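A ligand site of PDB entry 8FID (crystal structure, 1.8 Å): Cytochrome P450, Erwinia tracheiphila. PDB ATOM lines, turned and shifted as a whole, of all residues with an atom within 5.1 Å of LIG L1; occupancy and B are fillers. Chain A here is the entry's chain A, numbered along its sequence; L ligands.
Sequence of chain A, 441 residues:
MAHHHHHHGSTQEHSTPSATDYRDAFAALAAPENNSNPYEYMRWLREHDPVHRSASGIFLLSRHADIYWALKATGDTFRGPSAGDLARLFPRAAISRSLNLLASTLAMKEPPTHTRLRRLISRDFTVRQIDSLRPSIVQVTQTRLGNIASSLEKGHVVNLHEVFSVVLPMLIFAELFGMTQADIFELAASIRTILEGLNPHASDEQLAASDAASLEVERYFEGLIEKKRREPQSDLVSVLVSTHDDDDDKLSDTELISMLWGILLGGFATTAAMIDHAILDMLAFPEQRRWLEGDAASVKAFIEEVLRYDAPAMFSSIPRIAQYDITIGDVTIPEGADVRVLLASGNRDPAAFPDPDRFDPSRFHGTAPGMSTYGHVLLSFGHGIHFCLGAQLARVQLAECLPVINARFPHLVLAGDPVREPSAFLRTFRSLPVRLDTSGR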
ATOM      1  N   LEU A 102     -15.274  18.922  20.501  1.00  0.00           N
ATOM      2  CA  LEU A 102     -14.328  19.674  21.311  1.00  0.00           C
ATOM      3  C   LEU A 102     -13.183  20.229  20.463  1.00  0.00           C
ATOM      4  O   LEU A 102     -12.753  21.369  20.659  1.00  0.00           O
ATOM      5  CB  LEU A 102     -13.779  18.781  22.417  1.00  0.00           C
ATOM      6  CG  LEU A 102     -12.910  19.448  23.487  1.00  0.00           C
ATOM      7  CD1 LEU A 102     -13.739  20.388  24.357  1.00  0.00           C
ATOM      8  CD2 LEU A 102     -12.234  18.387  24.337  1.00  0.00           C
ATOM      9  N   THR A 105     -13.774  23.701  19.178  1.00  0.00           N
ATOM     10  CA  THR A 105     -14.101  24.817  20.062  1.00  0.00           C
ATOM     11  C   THR A 105     -12.901  25.771  20.149  1.00  0.00           C
ATOM     12  O   THR A 105     -11.762  25.389  19.900  1.00  0.00           O
ATOM     13  CB  THR A 105     -14.456  24.347  21.470  1.00  0.00           C
ATOM     14  OG1 THR A 105     -13.328  23.717  22.091  1.00  0.00           O
ATOM     15  CG2 THR A 105     -15.627  23.369  21.435  1.00  0.00           C
ATOM     16  N   LEU A 106     -13.189  27.022  20.520  1.00  0.00           N
ATOM     17  CA  LEU A 106     -12.131  28.018  20.585  1.00  0.00           C
ATOM     18  C   LEU A 106     -11.128  27.731  21.693  1.00  0.00           C
ATOM     19  O   LEU A 106     -10.009  28.267  21.645  1.00  0.00           O
ATOM     20  CB  LEU A 106     -12.729  29.404  20.784  1.00  0.00           C
ATOM     21  CG  LEU A 106     -13.198  29.812  22.194  1.00  0.00           C
ATOM     22  CD1 LEU A 106     -13.480  31.309  22.191  1.00  0.00           C
ATOM     23  CD2 LEU A 106     -14.419  29.039  22.638  1.00  0.00           C
ATOM     24  N   ALA A 107     -11.487  26.909  22.671  1.00  0.00           N
ATOM     25  CA  ALA A 107     -10.562  26.566  23.751  1.00  0.00           C
ATOM     26  C   ALA A 107      -9.386  25.729  23.250  1.00  0.00           C
ATOM     27  O   ALA A 107      -8.377  25.620  23.957  1.00  0.00           O
ATOM     28  CB  ALA A 107     -11.303  25.821  24.853  1.00  0.00           C
ATOM     29  N   LEU A 195     -20.530  15.975  29.642  1.00  0.00           N
ATOM     30  CA  LEU A 195     -19.426  16.517  30.419  1.00  0.00           C
ATOM     31  C   LEU A 195     -18.562  15.416  31.018  1.00  0.00           C
ATOM     32  O   LEU A 195     -17.336  15.529  31.035  1.00  0.00           O
ATOM     33  CB  LEU A 195     -19.974  17.429  31.514  1.00  0.00           C
ATOM     34  CG  LEU A 195     -20.524  18.792  31.076  1.00  0.00           C
ATOM     35  CD1 LEU A 195     -21.282  19.451  32.221  1.00  0.00           C
ATOM     36  CD2 LEU A 195     -19.399  19.699  30.590  1.00  0.00           C
ATOM     37  N   LEU A 198     -15.602  13.810  29.213  1.00  0.00           N
ATOM     38  CA  LEU A 198     -14.508  14.701  28.834  1.00  0.00           C
ATOM     39  C   LEU A 198     -13.412  14.724  29.911  1.00  0.00           C
ATOM     40  O   LEU A 198     -13.108  15.759  30.499  1.00  0.00           O
ATOM     41  CB  LEU A 198     -15.041  16.105  28.581  1.00  0.00           C
ATOM     42  CG  LEU A 198     -15.942  16.318  27.370  1.00  0.00           C
ATOM     43  CD1 LEU A 198     -16.467  17.738  27.382  1.00  0.00           C
ATOM     44  CD2 LEU A 198     -15.198  16.025  26.074  1.00  0.00           C
ATOM     45  N   MET A 259     -19.093  25.601  18.664  1.00  0.00           N
ATOM     46  CA  MET A 259     -19.367  26.734  19.530  1.00  0.00           C
ATOM     47  C   MET A 259     -20.687  26.552  20.274  1.00  0.00           C
ATOM     48  O   MET A 259     -20.765  26.757  21.486  1.00  0.00           O
ATOM     49  CB  MET A 259     -19.390  28.018  18.704  1.00  0.00           C
ATOM     50  CG  MET A 259     -19.594  29.290  19.514  1.00  0.00           C
ATOM     51  SD  MET A 259     -18.115  29.743  20.439  1.00  0.00           S
ATOM     52  CE  MET A 259     -17.211  30.640  19.180  1.00  0.00           C
ATOM     53  N   TRP A 261     -22.421  23.728  20.861  1.00  0.00           N
ATOM     54  CA  TRP A 261     -22.210  22.624  21.793  1.00  0.00           C
ATOM     55  C   TRP A 261     -21.355  23.053  22.967  1.00  0.00           C
ATOM     56  O   TRP A 261     -21.673  22.763  24.125  1.00  0.00           O
ATOM     57  CB  TRP A 261     -21.573  21.463  21.008  1.00  0.00           C
ATOM     58  CG  TRP A 261     -21.143  20.245  21.759  1.00  0.00           C
ATOM     59  CD1 TRP A 261     -21.893  19.143  22.053  1.00  0.00           C
ATOM     60  CD2 TRP A 261     -19.829  19.972  22.265  1.00  0.00           C
ATOM     61  NE1 TRP A 261     -21.135  18.217  22.716  1.00  0.00           N
ATOM     62  CE2 TRP A 261     -19.867  18.701  22.866  1.00  0.00           C
ATOM     63  CE3 TRP A 261     -18.625  20.686  22.272  1.00  0.00           C
ATOM     64  CZ2 TRP A 261     -18.744  18.124  23.457  1.00  0.00           C
ATOM     65  CZ3 TRP A 261     -17.510  20.114  22.867  1.00  0.00           C
ATOM     66  CH2 TRP A 261     -17.583  18.853  23.457  1.00  0.00           C
ATOM     67  N   GLY A 262     -20.262  23.769  22.694  1.00  0.00           N
ATOM     68  CA  GLY A 262     -19.319  24.111  23.744  1.00  0.00           C
ATOM     69  C   GLY A 262     -19.877  25.108  24.746  1.00  0.00           C
ATOM     70  O   GLY A 262     -19.801  24.902  25.963  1.00  0.00           O
ATOM     71  N   ILE A 263     -20.437  26.214  24.249  1.00  0.00           N
ATOM     72  CA  ILE A 263     -21.015  27.210  25.160  1.00  0.00           C
ATOM     73  C   ILE A 263     -22.108  26.576  26.009  1.00  0.00           C
ATOM     74  O   ILE A 263     -22.237  26.871  27.202  1.00  0.00           O
ATOM     75  CB  ILE A 263     -21.544  28.410  24.364  1.00  0.00           C
ATOM     76  CG1 ILE A 263     -20.433  29.087  23.563  1.00  0.00           C
ATOM     77  CG2 ILE A 263     -22.197  29.424  25.307  1.00  0.00           C
ATOM     78  CD1 ILE A 263     -19.359  29.723  24.412  1.00  0.00           C
ATOM     79  N   LEU A 265     -22.231  23.459  27.021  1.00  0.00           N
ATOM     80  CA  LEU A 265     -21.574  22.673  28.056  1.00  0.00           C
ATOM     81  C   LEU A 265     -21.083  23.561  29.199  1.00  0.00           C
ATOM     82  O   LEU A 265     -21.203  23.208  30.372  1.00  0.00           O
ATOM     83  CB  LEU A 265     -20.393  21.902  27.464  1.00  0.00           C
ATOM     84  CG  LEU A 265     -20.676  20.766  26.489  1.00  0.00           C
ATOM     85  CD1 LEU A 265     -19.399  19.967  26.279  1.00  0.00           C
ATOM     86  CD2 LEU A 265     -21.801  19.883  26.971  1.00  0.00           C
ATOM     87  N   GLY A 266     -20.513  24.705  28.871  1.00  0.00           N
ATOM     88  CA  GLY A 266     -19.977  25.578  29.895  1.00  0.00           C
ATOM     89  C   GLY A 266     -20.959  26.531  30.517  1.00  0.00           C
ATOM     90  O   GLY A 266     -20.617  27.234  31.470  1.00  0.00           O
ATOM     91  N   THR A 270     -21.165  24.397  35.808  1.00  0.00           N
ATOM     92  CA  THR A 270     -20.171  24.833  36.784  1.00  0.00           C
ATOM     93  C   THR A 270     -20.692  25.987  37.637  1.00  0.00           C
ATOM     94  O   THR A 270     -20.337  26.086  38.811  1.00  0.00           O
ATOM     95  CB  THR A 270     -18.893  25.258  36.076  1.00  0.00           C
ATOM     96  OG1 THR A 270     -19.230  26.061  34.933  1.00  0.00           O
ATOM     97  CG2 THR A 270     -18.081  24.038  35.638  1.00  0.00           C
ATOM     98  N   ALA A 313     -14.355  22.822  38.634  1.00  0.00           N
ATOM     99  CA  ALA A 313     -13.589  21.878  37.830  1.00  0.00           C
ATOM    100  C   ALA A 313     -12.203  21.727  38.444  1.00  0.00           C
ATOM    101  O   ALA A 313     -11.436  22.700  38.505  1.00  0.00           O
ATOM    102  CB  ALA A 313     -13.473  22.356  36.383  1.00  0.00           C
ATOM    103  N   PHE A 315      -9.588  19.929  37.332  1.00  0.00           N
ATOM    104  CA  PHE A 315      -8.728  20.265  36.201  1.00  0.00           C
ATOM    105  C   PHE A 315      -9.609  20.420  34.972  1.00  0.00           C
ATOM    106  O   PHE A 315     -10.810  20.112  34.997  1.00  0.00           O
ATOM    107  CB  PHE A 315      -7.641  19.208  35.972  1.00  0.00           C
ATOM    108  CG  PHE A 315      -8.169  17.829  35.709  1.00  0.00           C
ATOM    109  CD1 PHE A 315      -8.512  17.442  34.421  1.00  0.00           C
ATOM    110  CD2 PHE A 315      -8.313  16.931  36.737  1.00  0.00           C
ATOM    111  CE1 PHE A 315      -9.000  16.167  34.174  1.00  0.00           C
ATOM    112  CE2 PHE A 315      -8.796  15.664  36.491  1.00  0.00           C
ATOM    113  CZ  PHE A 315      -9.147  15.281  35.206  1.00  0.00           C
ATOM    114  N   SER A 316      -9.012  20.898  33.891  1.00  0.00           N
ATOM    115  CA  SER A 316      -9.735  21.214  32.675  1.00  0.00           C
ATOM    116  C   SER A 316      -9.674  20.059  31.683  1.00  0.00           C
ATOM    117  O   SER A 316      -8.628  19.406  31.538  1.00  0.00           O
ATOM    118  CB  SER A 316      -9.184  22.485  32.024  1.00  0.00           C
ATOM    119  OG  SER A 316      -9.882  22.772  30.828  1.00  0.00           O
ATOM    120  N   SER A 317     -10.789  19.819  31.001  1.00  0.00           N
ATOM    121  CA  SER A 317     -10.824  18.849  29.916  1.00  0.00           C
ATOM    122  C   SER A 317      -9.952  19.240  28.733  1.00  0.00           C
ATOM    123  O   SER A 317      -9.715  18.414  27.843  1.00  0.00           O
ATOM    124  CB  SER A 317     -12.257  18.652  29.420  1.00  0.00           C
ATOM    125  OG  SER A 317     -13.200  18.646  30.469  1.00  0.00           O
ATOM    126  N   ILE A 318      -9.471  20.480  28.678  1.00  0.00           N
ATOM    127  CA  ILE A 318      -8.780  20.993  27.501  1.00  0.00           C
ATOM    128  C   ILE A 318      -7.335  20.515  27.519  1.00  0.00           C
ATOM    129  O   ILE A 318      -6.594  20.826  28.459  1.00  0.00           O
ATOM    130  CB  ILE A 318      -8.845  22.529  27.438  1.00  0.00           C
ATOM    131  CG1 ILE A 318     -10.299  23.022  27.436  1.00  0.00           C
ATOM    132  CG2 ILE A 318      -8.100  23.037  26.216  1.00  0.00           C
ATOM    133  CD1 ILE A 318     -11.197  22.346  26.402  1.00  0.00           C
ATOM    134  N   PHE A 425     -13.576  14.672  37.537  1.00  0.00           N
ATOM    135  CA  PHE A 425     -12.950  15.982  37.541  1.00  0.00           C
ATOM    136  C   PHE A 425     -13.864  17.142  37.924  1.00  0.00           C
ATOM    137  O   PHE A 425     -13.369  18.213  38.279  1.00  0.00           O
ATOM    138  CB  PHE A 425     -12.328  16.253  36.153  1.00  0.00           C
ATOM    139  CG  PHE A 425     -13.331  16.584  35.076  1.00  0.00           C
ATOM    140  CD1 PHE A 425     -14.260  15.641  34.649  1.00  0.00           C
ATOM    141  CD2 PHE A 425     -13.314  17.812  34.449  1.00  0.00           C
ATOM    142  CE1 PHE A 425     -15.177  15.947  33.652  1.00  0.00           C
ATOM    143  CE2 PHE A 425     -14.212  18.129  33.451  1.00  0.00           C
ATOM    144  CZ  PHE A 425     -15.148  17.201  33.050  1.00  0.00           C
ATOM    145  N   LEU A 426     -15.178  16.969  37.859  1.00  0.00           N
ATOM    146  CA  LEU A 426     -16.100  18.042  38.223  1.00  0.00           C
ATOM    147  C   LEU A 426     -16.600  17.858  39.647  1.00  0.00           C
ATOM    148  O   LEU A 426     -16.828  16.728  40.102  1.00  0.00           O
ATOM    149  CB  LEU A 426     -17.291  18.099  37.260  1.00  0.00           C
ATOM    150  CG  LEU A 426     -16.947  18.519  35.833  1.00  0.00           C
ATOM    151  CD1 LEU A 426     -18.164  18.411  34.921  1.00  0.00           C
ATOM    152  CD2 LEU A 426     -16.371  19.934  35.799  1.00  0.00           C
HETATM  153  C1  LIG L   1     -15.724  25.204  27.895  1.00  0.00           C
HETATM  154  C2  LIG L   1     -15.535  23.460  25.600  1.00  0.00           C
HETATM  155  C3  LIG L   1     -14.487  25.194  26.988  1.00  0.00           C
HETATM  156  C4  LIG L   1     -16.802  26.414  24.531  1.00  0.00           C
HETATM  157  C5  LIG L   1     -13.228  22.538  31.577  1.00  0.00           C
HETATM  158  C6  LIG L   1     -16.407  21.701  29.571  1.00  0.00           C
HETATM  159  C7  LIG L   1     -15.830  20.912  30.759  1.00  0.00           C
HETATM  160  C8  LIG L   1     -15.645  21.800  31.991  1.00  0.00           C
HETATM  161  C9  LIG L   1     -14.731  22.988  31.712  1.00  0.00           C
HETATM  162  C10 LIG L   1     -15.345  23.753  30.527  1.00  0.00           C
HETATM  163  C11 LIG L   1     -14.635  25.048  30.182  1.00  0.00           C
HETATM  164  C12 LIG L   1     -15.439  25.893  29.215  1.00  0.00           C
HETATM  165  C13 LIG L   1     -16.280  23.768  28.119  1.00  0.00           C
HETATM  166  C14 LIG L   1     -16.454  23.039  26.766  1.00  0.00           C
HETATM  167  C15 LIG L   1     -15.103  24.920  25.630  1.00  0.00           C
HETATM  168  C16 LIG L   1     -16.280  25.846  25.616  1.00  0.00           C
HETATM  169  C17 LIG L   1     -16.723  26.037  27.042  1.00  0.00           C
HETATM  170  C18 LIG L   1     -14.754  23.850  32.942  1.00  0.00           C
HETATM  171  C19 LIG L   1     -14.208  22.411  28.663  1.00  0.00           C
HETATM  172  C20 LIG L   1     -15.520  22.904  29.197  1.00  0.00           C
HETATM  173  O1  LIG L   1     -12.387  23.376  31.148  1.00  0.00           O
HETATM  174  O2  LIG L   1     -12.930  21.373  31.908  1.00  0.00           O
HETATM  175  C1  LG2 L   2     -13.106  28.788  29.890  1.00  0.00           C
HETATM  176  C2  LG2 L   2     -14.311  27.446  34.391  1.00  0.00           C
HETATM  177  C3  LG2 L   2     -18.697  29.446  33.799  1.00  0.00           C
HETATM  178  C4  LG2 L   2     -17.778  29.907  29.057  1.00  0.00           C
HETATM  179  C5  LG2 L   2     -13.032  28.272  31.159  1.00  0.00           C
HETATM  180  C6  LG2 L   2     -11.871  27.634  31.781  1.00  0.00           C
HETATM  181  C7  LG2 L   2     -12.209  27.266  33.009  1.00  0.00           C
HETATM  182  C8  LG2 L   2     -13.591  27.656  33.240  1.00  0.00           C
HETATM  183  C9  LG2 L   2     -11.311  26.579  34.056  1.00  0.00           C
HETATM  184  C10 LG2 L   2     -10.498  27.457  31.119  1.00  0.00           C
HETATM  185  C11 LG2 L   2     -10.292  26.002  30.707  1.00  0.00           C
HETATM  186  C12 LG2 L   2      -8.872  25.828  30.204  1.00  0.00           C
HETATM  187  O1  LG2 L   2      -8.172  26.845  30.006  1.00  0.00           O
HETATM  188  O2  LG2 L   2      -8.456  24.659  29.992  1.00  0.00           O
HETATM  189  C13 LG2 L   2     -15.571  27.947  34.653  1.00  0.00           C
HETATM  190  C14 LG2 L   2     -16.201  28.019  35.945  1.00  0.00           C
HETATM  191  C15 LG2 L   2     -17.426  28.555  35.776  1.00  0.00           C
HETATM  192  C16 LG2 L   2     -17.583  28.865  34.370  1.00  0.00           C
HETATM  193  C17 LG2 L   2     -15.567  27.523  37.264  1.00  0.00           C
HETATM  194  C18 LG2 L   2     -18.516  28.885  36.822  1.00  0.00           C
HETATM  195  C19 LG2 L   2     -18.208  29.129  38.105  1.00  0.00           C
HETATM  196  C20 LG2 L   2     -18.842  29.730  32.468  1.00  0.00           C
HETATM  197  C21 LG2 L   2     -20.026  30.266  31.838  1.00  0.00           C
HETATM  198  C22 LG2 L   2     -19.797  30.391  30.524  1.00  0.00           C
HETATM  199  C23 LG2 L   2     -18.434  29.945  30.263  1.00  0.00           C
HETATM  200  C24 LG2 L   2     -21.318  30.629  32.600  1.00  0.00           C
HETATM  201  C25 LG2 L   2     -20.858  30.947  29.535  1.00  0.00           C
HETATM  202  C26 LG2 L   2     -20.692  30.901  28.215  1.00  0.00           C
HETATM  203  C27 LG2 L   2     -16.428  29.649  28.864  1.00  0.00           C
HETATM  204  C28 LG2 L   2     -15.719  29.713  27.608  1.00  0.00           C
HETATM  205  C29 LG2 L   2     -14.432  29.404  27.827  1.00  0.00           C
HETATM  206  C30 LG2 L   2     -14.266  29.146  29.243  1.00  0.00           C
HETATM  207  C31 LG2 L   2     -16.364  30.068  26.247  1.00  0.00           C
HETATM  208  C32 LG2 L   2     -13.321  29.358  26.760  1.00  0.00           C
HETATM  209  C33 LG2 L   2     -12.719  30.736  26.586  1.00  0.00           C
HETATM  210  C34 LG2 L   2     -11.616  30.704  25.545  1.00  0.00           C
HETATM  211  O3  LG2 L   2     -11.153  29.594  25.168  1.00  0.00           O
HETATM  212  O4  LG2 L   2     -11.193  31.797  25.090  1.00  0.00           O
HETATM  213  N1  LG2 L   2     -14.049  28.252  32.085  1.00  0.00           N
HETATM  214  N2  LG2 L   2     -16.437  28.465  33.695  1.00  0.00           N
HETATM  215  N3  LG2 L   2     -17.881  29.544  31.475  1.00  0.00           N
HETATM  216  N4  LG2 L   2     -15.499  29.314  29.841  1.00  0.00           N
HETATM  217 FE1  LG2 L   2     -15.877  29.203  31.896  1.00  0.00          FE
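O1 of LIG L1 lies within hydrogen-bond range of OG of Ser 316 (2.6 Å). The side-chain hydroxyl (OG) of Ser 317 lies within hydrogen-bond range of an oxygen (O2) of LIG L1, 3.1 Å away. The side-chain hydroxyl (OG) of Ser 316 lies within hydrogen-bond range of an oxygen (O2) of LG2 L2. N of Ser 317 lies within hydrogen-bond range of O2 of LIG L1 (2.8 Å).
The backbone NH (N) of Ile 318 sits close to the side-chain hydroxyl (OG) of Ser 316 (3.2 Å). The backbone carbonyl oxygen (O) of Leu 102 is in hydrogen-bond range of the side-chain hydroxyl (OG1) of Thr 105 (2.8 Å). OG of Ser 317 is in hydrogen-bond range of O of Leu 198.
CD1 of Leu 102 touches C2 of LIG L1, 3.8 Å away. CB of Ala 107 touches C3 of LIG L1 (3.9 Å). CD2 of Leu 195 touches C6 of LIG L1, at 3.7 Å. Gly 262 touches LIG L1. N of Ile 263 touches C4 of LIG L1, 3.7 Å away. Ala 313 touches LIG L1 (CB to C18, 3.96 Å). O of Phe 315 touches O2 of LIG L1, at 3.95 Å. CD1 of Ile 318 touches C19 of LIG L1, 3.8 Å away. Phe 425 touches LIG L1. Of the 20 residues printed, 11 come within 4 Å of LIG L1. The nearest printed residue that does not touch LIG L1 is Leu 106 (4.02 Å).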
